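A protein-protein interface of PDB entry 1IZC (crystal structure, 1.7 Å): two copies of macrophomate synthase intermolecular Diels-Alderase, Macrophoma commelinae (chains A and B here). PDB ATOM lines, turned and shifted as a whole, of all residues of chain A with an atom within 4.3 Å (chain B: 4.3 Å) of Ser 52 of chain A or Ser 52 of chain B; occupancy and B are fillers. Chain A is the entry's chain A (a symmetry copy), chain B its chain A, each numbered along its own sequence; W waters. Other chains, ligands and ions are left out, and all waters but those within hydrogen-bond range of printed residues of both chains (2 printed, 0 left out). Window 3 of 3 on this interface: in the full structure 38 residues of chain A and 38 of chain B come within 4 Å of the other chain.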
ATOM      1  N   HIS A  48       6.502 -10.044   0.945  1.00  0.00           N
ATOM      2  CA  HIS A  48       6.240  -9.750  -0.469  1.00  0.00           C
ATOM      3  C   HIS A  48       4.931 -10.401  -0.937  1.00  0.00           C
ATOM      4  O   HIS A  48       4.838 -11.629  -1.104  1.00  0.00           O
ATOM      5  CB  HIS A  48       7.492 -10.246  -1.228  1.00  0.00           C
ATOM      6  CG  HIS A  48       7.457 -10.103  -2.721  1.00  0.00           C
ATOM      7  ND1 HIS A  48       6.833  -9.056  -3.372  1.00  0.00           N
ATOM      8  CD2 HIS A  48       8.106 -10.804  -3.682  1.00  0.00           C
ATOM      9  CE1 HIS A  48       7.105  -9.118  -4.664  1.00  0.00           C
ATOM     10  NE2 HIS A  48       7.877 -10.170  -4.880  1.00  0.00           N
ATOM     11  N   ILE A  50       2.947  -8.521  -3.443  1.00  0.00           N
ATOM     12  CA  ILE A  50       2.629  -7.934  -4.753  1.00  0.00           C
ATOM     13  C   ILE A  50       3.171  -8.901  -5.800  1.00  0.00           C
ATOM     14  O   ILE A  50       4.381  -9.130  -5.865  1.00  0.00           O
ATOM     15  CB  ILE A  50       3.314  -6.566  -4.936  1.00  0.00           C
ATOM     16  CG1 ILE A  50       2.758  -5.566  -3.914  1.00  0.00           C
ATOM     17  CG2 ILE A  50       3.074  -6.053  -6.355  1.00  0.00           C
ATOM     18  CD1 ILE A  50       3.539  -4.248  -3.844  1.00  0.00           C
ATOM     19  N   PRO A  51       2.287  -9.467  -6.648  1.00  0.00           N
ATOM     20  CA  PRO A  51       2.701 -10.425  -7.677  1.00  0.00           C
ATOM     21  C   PRO A  51       3.382  -9.784  -8.869  1.00  0.00           C
ATOM     22  O   PRO A  51       2.819  -9.705  -9.964  1.00  0.00           O
ATOM     23  CB  PRO A  51       1.386 -11.110  -8.040  1.00  0.00           C
ATOM     24  CG  PRO A  51       0.415  -9.962  -7.980  1.00  0.00           C
ATOM     25  CD  PRO A  51       0.830  -9.222  -6.710  1.00  0.00           C
ATOM     26  N   SER A  52       4.611  -9.329  -8.644  1.00  0.00           N
ATOM     27  CA  SER A  52       5.382  -8.673  -9.691  1.00  0.00           C
ATOM     28  C   SER A  52       6.858  -8.962  -9.460  1.00  0.00           C
ATOM     29  O   SER A  52       7.397  -8.628  -8.398  1.00  0.00           O
ATOM     30  CB  SER A  52       5.146  -7.156  -9.628  1.00  0.00           C
ATOM     31  OG  SER A  52       6.128  -6.477 -10.385  1.00  0.00           O
ATOM     32  N   THR A  53       7.509  -9.588 -10.436  1.00  0.00           N
ATOM     33  CA  THR A  53       8.929  -9.871 -10.276  1.00  0.00           C
ATOM     34  C   THR A  53       9.720  -8.567 -10.280  1.00  0.00           C
ATOM     35  O   THR A  53      10.806  -8.510  -9.714  1.00  0.00           O
ATOM     36  CB  THR A  53       9.463 -10.805 -11.371  1.00  0.00           C
ATOM     37  OG1 THR A  53       9.265 -10.198 -12.649  1.00  0.00           O
ATOM     38  CG2 THR A  53       8.731 -12.143 -11.326  1.00  0.00           C
ATOM     39  N   PHE A  54       9.185  -7.514 -10.903  1.00  0.00           N
ATOM     40  CA  PHE A  54       9.886  -6.226 -10.906  1.00  0.00           C
ATOM     41  C   PHE A  54       9.972  -5.762  -9.450  1.00  0.00           C
ATOM     42  O   PHE A  54      11.009  -5.283  -8.996  1.00  0.00           O
ATOM     43  CB  PHE A  54       9.129  -5.199 -11.771  1.00  0.00           C
ATOM     44  CG  PHE A  54       9.874  -3.915 -11.984  1.00  0.00           C
ATOM     45  CD1 PHE A  54       9.941  -2.955 -10.985  1.00  0.00           C
ATOM     46  CD2 PHE A  54      10.535  -3.675 -13.196  1.00  0.00           C
ATOM     47  CE1 PHE A  54      10.662  -1.763 -11.183  1.00  0.00           C
ATOM     48  CE2 PHE A  54      11.249  -2.509 -13.405  1.00  0.00           C
ATOM     49  CZ  PHE A  54      11.319  -1.543 -12.402  1.00  0.00           C
ATOM     50  N   VAL A  55       8.877  -5.917  -8.707  1.00  0.00           N
ATOM     51  CA  VAL A  55       8.886  -5.549  -7.292  1.00  0.00           C
ATOM     52  C   VAL A  55       9.899  -6.417  -6.534  1.00  0.00           C
ATOM     53  O   VAL A  55      10.635  -5.920  -5.685  1.00  0.00           O
ATOM     54  CB  VAL A  55       7.483  -5.714  -6.668  1.00  0.00           C
ATOM     55  CG1 VAL A  55       7.548  -5.528  -5.140  1.00  0.00           C
ATOM     56  CG2 VAL A  55       6.546  -4.660  -7.259  1.00  0.00           C
ATOM     57  N   THR A  56       9.949  -7.713  -6.836  1.00  0.00           N
ATOM     58  CA  THR A  56      10.907  -8.571  -6.145  1.00  0.00           C
ATOM     59  C   THR A  56      12.314  -8.021  -6.355  1.00  0.00           C
ATOM     60  O   THR A  56      13.140  -8.020  -5.446  1.00  0.00           O
ATOM     61  CB  THR A  56      10.909 -10.008  -6.697  1.00  0.00           C
ATOM     62  OG1 THR A  56       9.566 -10.417  -6.979  1.00  0.00           O
ATOM     63  CG2 THR A  56      11.523 -10.956  -5.667  1.00  0.00           C
ATOM     64  N   HIS B  48       4.415   6.591 -10.928  1.00  0.00           N
ATOM     65  CA  HIS B  48       4.284   5.136 -11.072  1.00  0.00           C
ATOM     66  C   HIS B  48       5.193   4.605 -12.189  1.00  0.00           C
ATOM     67  O   HIS B  48       4.942   4.814 -13.388  1.00  0.00           O
ATOM     68  CB  HIS B  48       2.779   4.883 -11.316  1.00  0.00           C
ATOM     69  CG  HIS B  48       2.379   3.456 -11.546  1.00  0.00           C
ATOM     70  ND1 HIS B  48       2.995   2.384 -10.931  1.00  0.00           N
ATOM     71  CD2 HIS B  48       1.318   2.942 -12.215  1.00  0.00           C
ATOM     72  CE1 HIS B  48       2.326   1.277 -11.207  1.00  0.00           C
ATOM     73  NE2 HIS B  48       1.303   1.586 -11.985  1.00  0.00           N
ATOM     74  N   ILE B  50       6.677   1.247 -11.665  1.00  0.00           N
ATOM     75  CA  ILE B  50       6.698  -0.217 -11.533  1.00  0.00           C
ATOM     76  C   ILE B  50       5.647  -0.752 -12.500  1.00  0.00           C
ATOM     77  O   ILE B  50       4.458  -0.459 -12.348  1.00  0.00           O
ATOM     78  CB  ILE B  50       6.327  -0.656 -10.103  1.00  0.00           C
ATOM     79  CG1 ILE B  50       7.390  -0.157  -9.115  1.00  0.00           C
ATOM     80  CG2 ILE B  50       6.225  -2.179 -10.039  1.00  0.00           C
ATOM     81  CD1 ILE B  50       6.999  -0.325  -7.642  1.00  0.00           C
ATOM     82  N   PRO B  51       6.066  -1.560 -13.496  1.00  0.00           N
ATOM     83  CA  PRO B  51       5.141  -2.112 -14.490  1.00  0.00           C
ATOM     84  C   PRO B  51       4.290  -3.251 -13.968  1.00  0.00           C
ATOM     85  O   PRO B  51       4.486  -4.415 -14.329  1.00  0.00           O
ATOM     86  CB  PRO B  51       6.080  -2.536 -15.617  1.00  0.00           C
ATOM     87  CG  PRO B  51       7.260  -3.066 -14.848  1.00  0.00           C
ATOM     88  CD  PRO B  51       7.446  -2.032 -13.739  1.00  0.00           C
ATOM     89  N   SER B  52       3.334  -2.901 -13.113  1.00  0.00           N
ATOM     90  CA  SER B  52       2.450  -3.892 -12.515  1.00  0.00           C
ATOM     91  C   SER B  52       1.095  -3.245 -12.266  1.00  0.00           C
ATOM     92  O   SER B  52       1.007  -2.247 -11.541  1.00  0.00           O
ATOM     93  CB  SER B  52       3.039  -4.365 -11.177  1.00  0.00           C
ATOM     94  OG  SER B  52       2.057  -5.046 -10.423  1.00  0.00           O
ATOM     95  N   THR B  53       0.045  -3.797 -12.869  1.00  0.00           N
ATOM     96  CA  THR B  53      -1.279  -3.230 -12.650  1.00  0.00           C
ATOM     97  C   THR B  53      -1.706  -3.459 -11.203  1.00  0.00           C
ATOM     98  O   THR B  53      -2.517  -2.704 -10.679  1.00  0.00           O
ATOM     99  CB  THR B  53      -2.329  -3.822 -13.600  1.00  0.00           C
ATOM    100  OG1 THR B  53      -2.405  -5.234 -13.404  1.00  0.00           O
ATOM    101  CG2 THR B  53      -1.952  -3.530 -15.049  1.00  0.00           C
ATOM    102  N   PHE B  54      -1.162  -4.487 -10.547  1.00  0.00           N
ATOM    103  CA  PHE B  54      -1.510  -4.731  -9.143  1.00  0.00           C
ATOM    104  C   PHE B  54      -1.026  -3.516  -8.348  1.00  0.00           C
ATOM    105  O   PHE B  54      -1.730  -3.008  -7.476  1.00  0.00           O
ATOM    106  CB  PHE B  54      -0.843  -6.025  -8.637  1.00  0.00           C
ATOM    107  CG  PHE B  54      -1.298  -6.452  -7.273  1.00  0.00           C
ATOM    108  CD1 PHE B  54      -0.824  -5.817  -6.134  1.00  0.00           C
ATOM    109  CD2 PHE B  54      -2.229  -7.489  -7.131  1.00  0.00           C
ATOM    110  CE1 PHE B  54      -1.273  -6.206  -4.858  1.00  0.00           C
ATOM    111  CE2 PHE B  54      -2.680  -7.881  -5.884  1.00  0.00           C
ATOM    112  CZ  PHE B  54      -2.208  -7.243  -4.738  1.00  0.00           C
ATOM    113  N   VAL B  55       0.178  -3.038  -8.657  1.00  0.00           N
ATOM    114  CA  VAL B  55       0.696  -1.849  -7.983  1.00  0.00           C
ATOM    115  C   VAL B  55      -0.203  -0.643  -8.288  1.00  0.00           C
ATOM    116  O   VAL B  55      -0.501   0.153  -7.402  1.00  0.00           O
ATOM    117  CB  VAL B  55       2.144  -1.549  -8.425  1.00  0.00           C
ATOM    118  CG1 VAL B  55       2.604  -0.185  -7.875  1.00  0.00           C
ATOM    119  CG2 VAL B  55       3.069  -2.641  -7.887  1.00  0.00           C
ATOM    120  N   THR B  56      -0.644  -0.502  -9.537  1.00  0.00           N
ATOM    121  CA  THR B  56      -1.511   0.625  -9.865  1.00  0.00           C
ATOM    122  C   THR B  56      -2.745   0.586  -8.970  1.00  0.00           C
ATOM    123  O   THR B  56      -3.223   1.615  -8.498  1.00  0.00           O
ATOM    124  CB  THR B  56      -2.019   0.568 -11.317  1.00  0.00           C
ATOM    125  OG1 THR B  56      -0.964   0.124 -12.179  1.00  0.00           O
ATOM    126  CG2 THR B  56      -2.484   1.956 -11.756  1.00  0.00           C
HETATM  127  O   HOH W   1       1.757  -7.586 -11.233  1.00  0.00           O
HETATM  128  O   HOH W   2       5.562  -6.495 -13.007  1.00  0.00           O
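Of the 8 printed residues of chain B, 5 touch a printed residue of chain A.
Hydrophobic or aromatic side chains of chain B that line the printed part of chain A: Ile 50, Pro 51, Phe 54 and Val 55.
Among the printed residues, 7 pairs touch across the chains.
Water W1 bridges the side-chain hydroxyl of Ser 52 of chain B (2.7 Å) and the backbone carbonyl oxygen of Pro 51 of chain A (2.7 Å).
Water W2 lies within hydrogen-bond range of OG of Ser 52 of chain A and O of Pro 51 of chain B.
O of Ile 50 of chain B sits close to ND1 of His 48 of chain B, 3.5 Å away.
OG1 of Thr 56 of chain A lies within hydrogen-bond range of O of Ser 52 of chain A, at 3.1 Å.
N of Phe 54 of chain A sits close to OG of Ser 52 of chain A (3.3 Å).
OG of Ser 52 of chain B lies within hydrogen-bond range of N of Val 55 of chain B, 3.3 Å away.
The side-chain hydroxyl of Ser 52 of chain B sits close to the backbone NH of Phe 54 of chain B, at 3.3 Å.
O of Ser 52 of chain B is in hydrogen-bond range of OG1 of Thr 56 of chain B (3.1 Å).
CG2 of Ile 50 of chain A touches CD1 of Phe 54 of chain B, 3.9 Å away.
Val 55 of chain B touches Ile 50 of chain A (CG2 to CG2, 3.7 Å).
Pro 51 of chain A touches Phe 54 of chain B.
Ser 52 of chain A touches Ser 52 of chain B (CB to OG, 3.8 Å).
Phe 54 of chain A touches Ile 50 of chain B.
Phe 54 of chain A touches Pro 51 of chain B (CG to CD, 3.5 Å).
Ile 50 of chain B touches Val 55 of chain A (CG2 to CG2, 3.7 Å).
Ile 50 of chain A touches Phe 54 of chain B, and with the chains exchanged Phe 54 of chain A touches Ile 50 of chain B.
Ile 50 of chain A touches Val 55 of chain B, and with the chains exchanged Val 55 of chain A touches Ile 50 of chain B.
Pro 51 of chain A touches Phe 54 of chain B, and with the chains exchanged Phe 54 of chain A touches Pro 51 of chain B.
Ser 52 of chain A touches its own counterpart, Ser 52 of chain B.
Positions printed for both chains: 48, 50, 51, 52, 53, 54, 55 and 56.
Of the 7 pairs that touch across the chains among the printed residues, 7 have their exchanged pair printed and touching as well.
Of the printed residues of chain B, Pro 51 of chain A touches Phe 54 (3.5 Å).
Printed residues of chain A within 4 Å of Ile 50 of chain B: Phe 54 and Val 55.
Of the printed residues of chain A, Pro 51 of chain B touches Phe 54 (3.5 Å).
Ser 52 of chain B touches just one residue of chain A: Ser 52 (3.8 Å).
Printed residues of chain A within 4 Å of Val 55 of chain B: Ile 50 (3.7 Å).
The nearest printed residue of chain B that does not touch Ser 52 of chain A is Ile 50 of chain B (4.3 Å).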
